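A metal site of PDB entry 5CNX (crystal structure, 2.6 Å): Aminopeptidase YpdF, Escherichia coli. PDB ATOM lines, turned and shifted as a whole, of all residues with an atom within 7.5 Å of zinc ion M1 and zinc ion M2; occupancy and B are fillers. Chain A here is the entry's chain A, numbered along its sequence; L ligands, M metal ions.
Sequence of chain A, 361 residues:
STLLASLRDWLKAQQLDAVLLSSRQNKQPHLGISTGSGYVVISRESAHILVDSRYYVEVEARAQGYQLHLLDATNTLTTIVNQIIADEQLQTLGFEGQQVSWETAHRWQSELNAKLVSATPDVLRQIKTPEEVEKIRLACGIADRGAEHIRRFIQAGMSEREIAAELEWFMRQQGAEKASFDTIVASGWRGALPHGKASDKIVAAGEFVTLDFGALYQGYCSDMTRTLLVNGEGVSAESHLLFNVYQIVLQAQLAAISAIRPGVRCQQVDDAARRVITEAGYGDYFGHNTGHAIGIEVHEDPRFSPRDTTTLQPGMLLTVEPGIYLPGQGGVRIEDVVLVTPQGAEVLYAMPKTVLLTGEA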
ATOM      1  N   PHE A 181       3.731   4.095  25.338  1.00  0.00           N
ATOM      2  CA  PHE A 181       2.836   2.956  25.518  1.00  0.00           C
ATOM      3  C   PHE A 181       2.865   2.502  26.974  1.00  0.00           C
ATOM      4  O   PHE A 181       3.750   2.906  27.722  1.00  0.00           O
ATOM      5  CB  PHE A 181       3.230   1.791  24.608  1.00  0.00           C
ATOM      6  CG  PHE A 181       4.637   1.315  24.799  1.00  0.00           C
ATOM      7  CD1 PHE A 181       4.926   0.308  25.722  1.00  0.00           C
ATOM      8  CD2 PHE A 181       5.681   1.908  24.085  1.00  0.00           C
ATOM      9  CE1 PHE A 181       6.215  -0.136  25.927  1.00  0.00           C
ATOM     10  CE2 PHE A 181       6.996   1.474  24.283  1.00  0.00           C
ATOM     11  CZ  PHE A 181       7.259   0.435  25.211  1.00  0.00           C
ATOM     12  N   ILE A 184       5.846  -1.839  30.657  1.00  0.00           N
ATOM     13  CA  ILE A 184       5.963  -3.227  31.086  1.00  0.00           C
ATOM     14  C   ILE A 184       7.057  -3.331  32.134  1.00  0.00           C
ATOM     15  O   ILE A 184       8.199  -2.943  31.883  1.00  0.00           O
ATOM     16  CB  ILE A 184       6.291  -4.161  29.917  1.00  0.00           C
ATOM     17  CG1 ILE A 184       5.075  -4.307  28.991  1.00  0.00           C
ATOM     18  CG2 ILE A 184       6.749  -5.516  30.426  1.00  0.00           C
ATOM     19  CD1 ILE A 184       5.424  -4.922  27.657  1.00  0.00           C
ATOM     20  N   PRO A 194       5.621 -11.630  27.963  1.00  0.00           N
ATOM     21  CA  PRO A 194       6.236 -10.582  27.115  1.00  0.00           C
ATOM     22  C   PRO A 194       5.572  -9.205  27.213  1.00  0.00           C
ATOM     23  O   PRO A 194       6.231  -8.184  26.988  1.00  0.00           O
ATOM     24  CB  PRO A 194       6.080 -11.152  25.695  1.00  0.00           C
ATOM     25  CG  PRO A 194       5.989 -12.629  25.889  1.00  0.00           C
ATOM     26  CD  PRO A 194       5.241 -12.823  27.187  1.00  0.00           C
ATOM     27  N   HIS A 195       4.289  -9.179  27.581  1.00  0.00           N
ATOM     28  CA  HIS A 195       3.545  -7.929  27.723  1.00  0.00           C
ATOM     29  C   HIS A 195       2.986  -7.744  29.102  1.00  0.00           C
ATOM     30  O   HIS A 195       1.913  -7.168  29.271  1.00  0.00           O
ATOM     31  CB  HIS A 195       2.416  -7.858  26.700  1.00  0.00           C
ATOM     32  CG  HIS A 195       2.873  -7.358  25.368  1.00  0.00           C
ATOM     33  ND1 HIS A 195       2.838  -6.018  25.042  1.00  0.00           N
ATOM     34  CD2 HIS A 195       3.441  -7.986  24.310  1.00  0.00           C
ATOM     35  CE1 HIS A 195       3.328  -5.845  23.833  1.00  0.00           C
ATOM     36  NE2 HIS A 195       3.710  -7.024  23.368  1.00  0.00           N
ATOM     37  N   LEU A 211      12.125  -4.317  31.959  1.00  0.00           N
ATOM     38  CA  LEU A 211      11.438  -3.045  31.789  1.00  0.00           C
ATOM     39  C   LEU A 211      11.321  -2.702  30.303  1.00  0.00           C
ATOM     40  O   LEU A 211      12.318  -2.433  29.646  1.00  0.00           O
ATOM     41  CB  LEU A 211      12.159  -1.908  32.532  1.00  0.00           C
ATOM     42  CG  LEU A 211      12.283  -2.069  34.054  1.00  0.00           C
ATOM     43  CD1 LEU A 211      13.681  -2.539  34.442  1.00  0.00           C
ATOM     44  CD2 LEU A 211      11.918  -0.772  34.779  1.00  0.00           C
ATOM     45  N   ASP A 212      10.092  -2.749  29.807  1.00  0.00           N
ATOM     46  CA  ASP A 212       9.762  -2.359  28.453  1.00  0.00           C
ATOM     47  C   ASP A 212       8.911  -1.095  28.497  1.00  0.00           C
ATOM     48  O   ASP A 212       7.814  -1.099  29.072  1.00  0.00           O
ATOM     49  CB  ASP A 212       9.023  -3.486  27.748  1.00  0.00           C
ATOM     50  CG  ASP A 212       8.967  -3.330  26.245  1.00  0.00           C
ATOM     51  OD1 ASP A 212       9.041  -2.178  25.740  1.00  0.00           O
ATOM     52  OD2 ASP A 212       8.837  -4.378  25.578  1.00  0.00           O
ATOM     53  N   PHE A 213       9.413  -0.036  27.874  1.00  0.00           N
ATOM     54  CA  PHE A 213       8.822   1.282  28.048  1.00  0.00           C
ATOM     55  C   PHE A 213       9.307   2.227  26.943  1.00  0.00           C
ATOM     56  O   PHE A 213      10.184   1.886  26.149  1.00  0.00           O
ATOM     57  CB  PHE A 213       9.209   1.841  29.408  1.00  0.00           C
ATOM     58  CG  PHE A 213      10.675   2.083  29.555  1.00  0.00           C
ATOM     59  CD1 PHE A 213      11.531   1.037  29.796  1.00  0.00           C
ATOM     60  CD2 PHE A 213      11.206   3.353  29.369  1.00  0.00           C
ATOM     61  CE1 PHE A 213      12.895   1.254  29.899  1.00  0.00           C
ATOM     62  CE2 PHE A 213      12.552   3.570  29.462  1.00  0.00           C
ATOM     63  CZ  PHE A 213      13.395   2.517  29.731  1.00  0.00           C
ATOM     64  N   GLY A 214       8.754   3.438  26.906  1.00  0.00           N
ATOM     65  CA  GLY A 214       9.137   4.366  25.869  1.00  0.00           C
ATOM     66  C   GLY A 214       8.568   5.735  26.090  1.00  0.00           C
ATOM     67  O   GLY A 214       7.663   5.926  26.912  1.00  0.00           O
ATOM     68  N   SER A 222       9.840   6.551  21.271  1.00  0.00           N
ATOM     69  CA  SER A 222      10.954   5.673  21.563  1.00  0.00           C
ATOM     70  C   SER A 222      10.382   4.409  22.207  1.00  0.00           C
ATOM     71  O   SER A 222       9.229   4.393  22.628  1.00  0.00           O
ATOM     72  CB  SER A 222      11.985   6.341  22.475  1.00  0.00           C
ATOM     73  OG  SER A 222      11.402   6.763  23.688  1.00  0.00           O
ATOM     74  N   ASP A 223      11.204   3.368  22.275  1.00  0.00           N
ATOM     75  CA  ASP A 223      10.767   2.052  22.717  1.00  0.00           C
ATOM     76  C   ASP A 223      11.995   1.304  23.209  1.00  0.00           C
ATOM     77  O   ASP A 223      12.879   0.996  22.401  1.00  0.00           O
ATOM     78  CB  ASP A 223      10.092   1.328  21.543  1.00  0.00           C
ATOM     79  CG  ASP A 223       9.432   0.038  21.938  1.00  0.00           C
ATOM     80  OD1 ASP A 223       9.509  -0.304  23.128  1.00  0.00           O
ATOM     81  OD2 ASP A 223       8.829  -0.624  21.068  1.00  0.00           O
ATOM     82  N   MET A 224      12.102   1.057  24.518  1.00  0.00           N
ATOM     83  CA  MET A 224      13.287   0.368  25.055  1.00  0.00           C
ATOM     84  C   MET A 224      12.970  -0.783  26.040  1.00  0.00           C
ATOM     85  O   MET A 224      12.046  -0.687  26.853  1.00  0.00           O
ATOM     86  CB  MET A 224      14.219   1.374  25.751  1.00  0.00           C
ATOM     87  CG  MET A 224      15.597   0.788  26.063  1.00  0.00           C
ATOM     88  SD  MET A 224      16.898   1.973  26.546  1.00  0.00           S
ATOM     89  CE  MET A 224      15.899   2.968  27.606  1.00  0.00           C
ATOM     90  N   THR A 225      13.747  -1.866  25.951  1.00  0.00           N
ATOM     91  CA  THR A 225      13.704  -2.898  26.975  1.00  0.00           C
ATOM     92  C   THR A 225      15.081  -3.204  27.544  1.00  0.00           C
ATOM     93  O   THR A 225      16.041  -3.394  26.790  1.00  0.00           O
ATOM     94  CB  THR A 225      13.099  -4.236  26.484  1.00  0.00           C
ATOM     95  OG1 THR A 225      11.786  -4.022  25.964  1.00  0.00           O
ATOM     96  CG2 THR A 225      12.993  -5.201  27.613  1.00  0.00           C
ATOM     97  N   THR A 290      11.268 -10.209  15.835  1.00  0.00           N
ATOM     98  CA  THR A 290      12.539  -9.695  16.331  1.00  0.00           C
ATOM     99  C   THR A 290      12.447  -8.175  16.545  1.00  0.00           C
ATOM    100  O   THR A 290      13.104  -7.617  17.438  1.00  0.00           O
ATOM    101  CB  THR A 290      13.696 -10.042  15.360  1.00  0.00           C
ATOM    102  OG1 THR A 290      13.911 -11.457  15.373  1.00  0.00           O
ATOM    103  CG2 THR A 290      14.993  -9.344  15.745  1.00  0.00           C
ATOM    104  N   GLY A 291      11.607  -7.499  15.770  1.00  0.00           N
ATOM    105  CA  GLY A 291      11.440  -6.074  15.974  1.00  0.00           C
ATOM    106  C   GLY A 291      10.396  -5.437  15.067  1.00  0.00           C
ATOM    107  O   GLY A 291       9.688  -6.133  14.316  1.00  0.00           O
ATOM    108  N   HIS A 292      10.269  -4.119  15.165  1.00  0.00           N
ATOM    109  CA  HIS A 292       9.290  -3.391  14.379  1.00  0.00           C
ATOM    110  C   HIS A 292       9.800  -1.996  14.083  1.00  0.00           C
ATOM    111  O   HIS A 292      10.609  -1.436  14.832  1.00  0.00           O
ATOM    112  CB  HIS A 292       7.961  -3.317  15.126  1.00  0.00           C
ATOM    113  CG  HIS A 292       8.092  -2.766  16.506  1.00  0.00           C
ATOM    114  ND1 HIS A 292       8.121  -1.413  16.763  1.00  0.00           N
ATOM    115  CD2 HIS A 292       8.198  -3.381  17.695  1.00  0.00           C
ATOM    116  CE1 HIS A 292       8.250  -1.219  18.068  1.00  0.00           C
ATOM    117  NE2 HIS A 292       8.291  -2.397  18.654  1.00  0.00           N
ATOM    118  N   ALA A 293       9.319  -1.416  12.993  1.00  0.00           N
ATOM    119  CA  ALA A 293       9.656  -0.025  12.709  1.00  0.00           C
ATOM    120  C   ALA A 293       8.975   0.862  13.754  1.00  0.00           C
ATOM    121  O   ALA A 293       8.006   0.445  14.417  1.00  0.00           O
ATOM    122  CB  ALA A 293       9.246   0.366  11.315  1.00  0.00           C
ATOM    123  N   ILE A 294       9.471   2.091  13.904  1.00  0.00           N
ATOM    124  CA  ILE A 294       8.921   3.008  14.892  1.00  0.00           C
ATOM    125  C   ILE A 294       9.030   4.423  14.349  1.00  0.00           C
ATOM    126  O   ILE A 294       9.910   4.706  13.549  1.00  0.00           O
ATOM    127  CB  ILE A 294       9.639   2.886  16.261  1.00  0.00           C
ATOM    128  CG1 ILE A 294       9.006   3.810  17.304  1.00  0.00           C
ATOM    129  CG2 ILE A 294      11.131   3.180  16.113  1.00  0.00           C
ATOM    130  CD1 ILE A 294       9.427   3.503  18.721  1.00  0.00           C
ATOM    131  N   VAL A 298       4.409   3.765  17.662  1.00  0.00           N
ATOM    132  CA  VAL A 298       5.305   2.784  18.271  1.00  0.00           C
ATOM    133  C   VAL A 298       5.516   1.581  17.346  1.00  0.00           C
ATOM    134  O   VAL A 298       6.639   1.091  17.235  1.00  0.00           O
ATOM    135  CB  VAL A 298       4.778   2.355  19.654  1.00  0.00           C
ATOM    136  CG1 VAL A 298       5.343   1.012  20.108  1.00  0.00           C
ATOM    137  CG2 VAL A 298       5.029   3.457  20.684  1.00  0.00           C
ATOM    138  N   HIS A 299       4.452   1.105  16.707  1.00  0.00           N
ATOM    139  CA  HIS A 299       4.587   0.001  15.757  1.00  0.00           C
ATOM    140  C   HIS A 299       4.306   0.442  14.333  1.00  0.00           C
ATOM    141  O   HIS A 299       3.184   0.794  13.993  1.00  0.00           O
ATOM    142  CB  HIS A 299       3.645  -1.134  16.140  1.00  0.00           C
ATOM    143  CG  HIS A 299       3.882  -1.653  17.515  1.00  0.00           C
ATOM    144  ND1 HIS A 299       3.080  -1.314  18.584  1.00  0.00           N
ATOM    145  CD2 HIS A 299       4.841  -2.469  18.006  1.00  0.00           C
ATOM    146  CE1 HIS A 299       3.537  -1.912  19.676  1.00  0.00           C
ATOM    147  NE2 HIS A 299       4.598  -2.615  19.348  1.00  0.00           N
ATOM    148  N   THR A 319      13.118  -1.484  15.807  1.00  0.00           N
ATOM    149  CA  THR A 319      13.588  -2.025  17.076  1.00  0.00           C
ATOM    150  C   THR A 319      14.203  -3.393  16.853  1.00  0.00           C
ATOM    151  O   THR A 319      13.869  -4.075  15.871  1.00  0.00           O
ATOM    152  CB  THR A 319      12.460  -2.137  18.130  1.00  0.00           C
ATOM    153  OG1 THR A 319      11.454  -3.072  17.694  1.00  0.00           O
ATOM    154  CG2 THR A 319      11.823  -0.764  18.397  1.00  0.00           C
ATOM    155  N   VAL A 320      15.144  -3.770  17.728  1.00  0.00           N
ATOM    156  CA  VAL A 320      15.659  -5.145  17.791  1.00  0.00           C
ATOM    157  C   VAL A 320      15.459  -5.673  19.210  1.00  0.00           C
ATOM    158  O   VAL A 320      16.153  -5.230  20.136  1.00  0.00           O
ATOM    159  CB  VAL A 320      17.139  -5.252  17.429  1.00  0.00           C
ATOM    160  CG1 VAL A 320      17.607  -6.702  17.562  1.00  0.00           C
ATOM    161  CG2 VAL A 320      17.420  -4.701  16.028  1.00  0.00           C
ATOM    162  N   GLU A 321      14.494  -6.580  19.381  1.00  0.00           N
ATOM    163  CA  GLU A 321      14.061  -7.004  20.712  1.00  0.00           C
ATOM    164  C   GLU A 321      13.714  -8.485  20.836  1.00  0.00           C
ATOM    165  O   GLU A 321      12.573  -8.849  21.130  1.00  0.00           O
ATOM    166  CB  GLU A 321      12.851  -6.171  21.117  1.00  0.00           C
ATOM    167  CG  GLU A 321      11.851  -5.992  19.998  1.00  0.00           C
ATOM    168  CD  GLU A 321      10.598  -5.285  20.440  1.00  0.00           C
ATOM    169  OE1 GLU A 321      10.174  -5.474  21.606  1.00  0.00           O
ATOM    170  OE2 GLU A 321      10.045  -4.527  19.632  1.00  0.00           O
ATOM    171  N   ARG A 333      14.315 -10.134  27.885  1.00  0.00           N
ATOM    172  CA  ARG A 333      14.249  -9.409  26.621  1.00  0.00           C
ATOM    173  C   ARG A 333      15.165  -8.202  26.669  1.00  0.00           C
ATOM    174  O   ARG A 333      15.297  -7.561  27.716  1.00  0.00           O
ATOM    175  CB  ARG A 333      12.815  -8.963  26.303  1.00  0.00           C
ATOM    176  CG  ARG A 333      12.713  -8.146  25.004  1.00  0.00           C
ATOM    177  CD  ARG A 333      11.277  -7.918  24.549  1.00  0.00           C
ATOM    178  NE  ARG A 333      10.531  -7.126  25.522  1.00  0.00           N
ATOM    179  CZ  ARG A 333       9.691  -7.657  26.411  1.00  0.00           C
ATOM    180  NH1 ARG A 333       9.493  -8.969  26.425  1.00  0.00           N
ATOM    181  NH2 ARG A 333       9.044  -6.885  27.276  1.00  0.00           N
ATOM    182  N   GLU A 335      15.918  -4.749  24.257  1.00  0.00           N
ATOM    183  CA  GLU A 335      15.438  -3.993  23.104  1.00  0.00           C
ATOM    184  C   GLU A 335      16.178  -2.684  22.840  1.00  0.00           C
ATOM    185  O   GLU A 335      16.332  -1.852  23.740  1.00  0.00           O
ATOM    186  CB  GLU A 335      13.939  -3.722  23.264  1.00  0.00           C
ATOM    187  CG  GLU A 335      13.322  -2.812  22.211  1.00  0.00           C
ATOM    188  CD  GLU A 335      11.795  -2.782  22.351  1.00  0.00           C
ATOM    189  OE1 GLU A 335      11.298  -2.984  23.484  1.00  0.00           O
ATOM    190  OE2 GLU A 335      11.116  -2.526  21.331  1.00  0.00           O
ATOM    191  N   ASP A 336      16.617  -2.519  21.599  1.00  0.00           N
ATOM    192  CA  ASP A 336      17.208  -1.270  21.139  1.00  0.00           C
ATOM    193  C   ASP A 336      16.382  -0.694  19.999  1.00  0.00           C
ATOM    194  O   ASP A 336      15.740  -1.442  19.247  1.00  0.00           O
ATOM    195  CB  ASP A 336      18.633  -1.479  20.639  1.00  0.00           C
ATOM    196  CG  ASP A 336      19.628  -1.642  21.768  1.00  0.00           C
ATOM    197  OD1 ASP A 336      19.442  -0.996  22.825  1.00  0.00           O
ATOM    198  OD2 ASP A 336      20.612  -2.388  21.568  1.00  0.00           O
ATOM    199  N   VAL A 337      16.383   0.632  19.867  1.00  0.00           N
ATOM    200  CA  VAL A 337      15.934   1.256  18.626  1.00  0.00           C
ATOM    201  C   VAL A 337      17.174   1.450  17.753  1.00  0.00           C
ATOM    202  O   VAL A 337      18.187   1.980  18.205  1.00  0.00           O
ATOM    203  CB  VAL A 337      15.232   2.605  18.843  1.00  0.00           C
ATOM    204  CG1 VAL A 337      15.176   3.400  17.540  1.00  0.00           C
ATOM    205  CG2 VAL A 337      13.829   2.393  19.395  1.00  0.00           C
HETATM  206 AS1  LIG L   1       6.633  -3.236  22.374  1.00  0.00          AS
HETATM  207  O1  LIG L   1       8.370  -3.101  22.377  1.00  0.00           O
HETATM  208  O2  LIG L   1       5.870  -1.690  22.141  1.00  0.00           O
HETATM  209  C1  LIG L   1       6.132  -4.524  20.969  1.00  0.00           C
HETATM  210  C2  LIG L   1       6.024  -3.916  24.110  1.00  0.00           C
HETATM  211 ZN    ZN M   1       9.517  -2.363  23.726  1.00  0.00          ZN
HETATM  212 ZN    ZN M   2       9.237  -2.790  20.561  1.00  0.00          ZN
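Phe 181 touches zinc ion M1 (CZ to ZN, 3.9 Å). OG1 of Thr 225 touches zinc ion M1, at 3.6 Å. Of the 26 residues printed, 6 come within 4 Å of zinc ion M1.
Zinc ion M2 is bound by O1 of the ligand, OE2 of Glu 335, OE2 of Glu 321, NE2 of His 292 and OD2 of Asp 223. Zinc ion M2 has five donor atoms within binding distance.
O of Thr 225 is in hydrogen-bond range of N of Glu 335, 2.9 Å away. The side-chain carboxylate (OD2) of Asp 212 lies close to the side-chain hydroxyl (OG1) of Thr 225, 3.0 Å away. The guanidinium group of Arg 333 is in salt-bridge range of the side-chain carboxylate of Asp 212. N of Ile 184 sits at hydrogen-bond distance from O of Asp 212, at 2.6 Å. The backbone carbonyl oxygen (O) of Thr 290 is in hydrogen-bond range of the backbone NH (N) of Glu 321, 2.6 Å away. The backbone NH (N) of Thr 319 is in hydrogen-bond range of the backbone carbonyl oxygen (O) of His 292, at 2.7 Å. O of Val 298 lies close to ND1 of His 292, 2.9 Å away. The side-chain hydroxyl (OG1) of Thr 225 sits at hydrogen-bond distance from the guanidinium group (NE) of Arg 333, 3.4 Å away.
Thr 319 touches zinc ion M2. The nearest printed residue that does not touch zinc ion M2 is His 299 (4.8 Å).
Zinc ion M1 is bound by the side-chain carboxylate of Glu 335 (1.9 Å), an oxygen (O1) of the ligand (1.9 Å), the side-chain carboxylate of Asp 212 (2.1 Å) and the side-chain carboxylate of Asp 223 (2.1 Å). Slightly farther from zinc ion M1 lies the side-chain carboxylate (OD2) of Asp 212 (2.8 Å).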
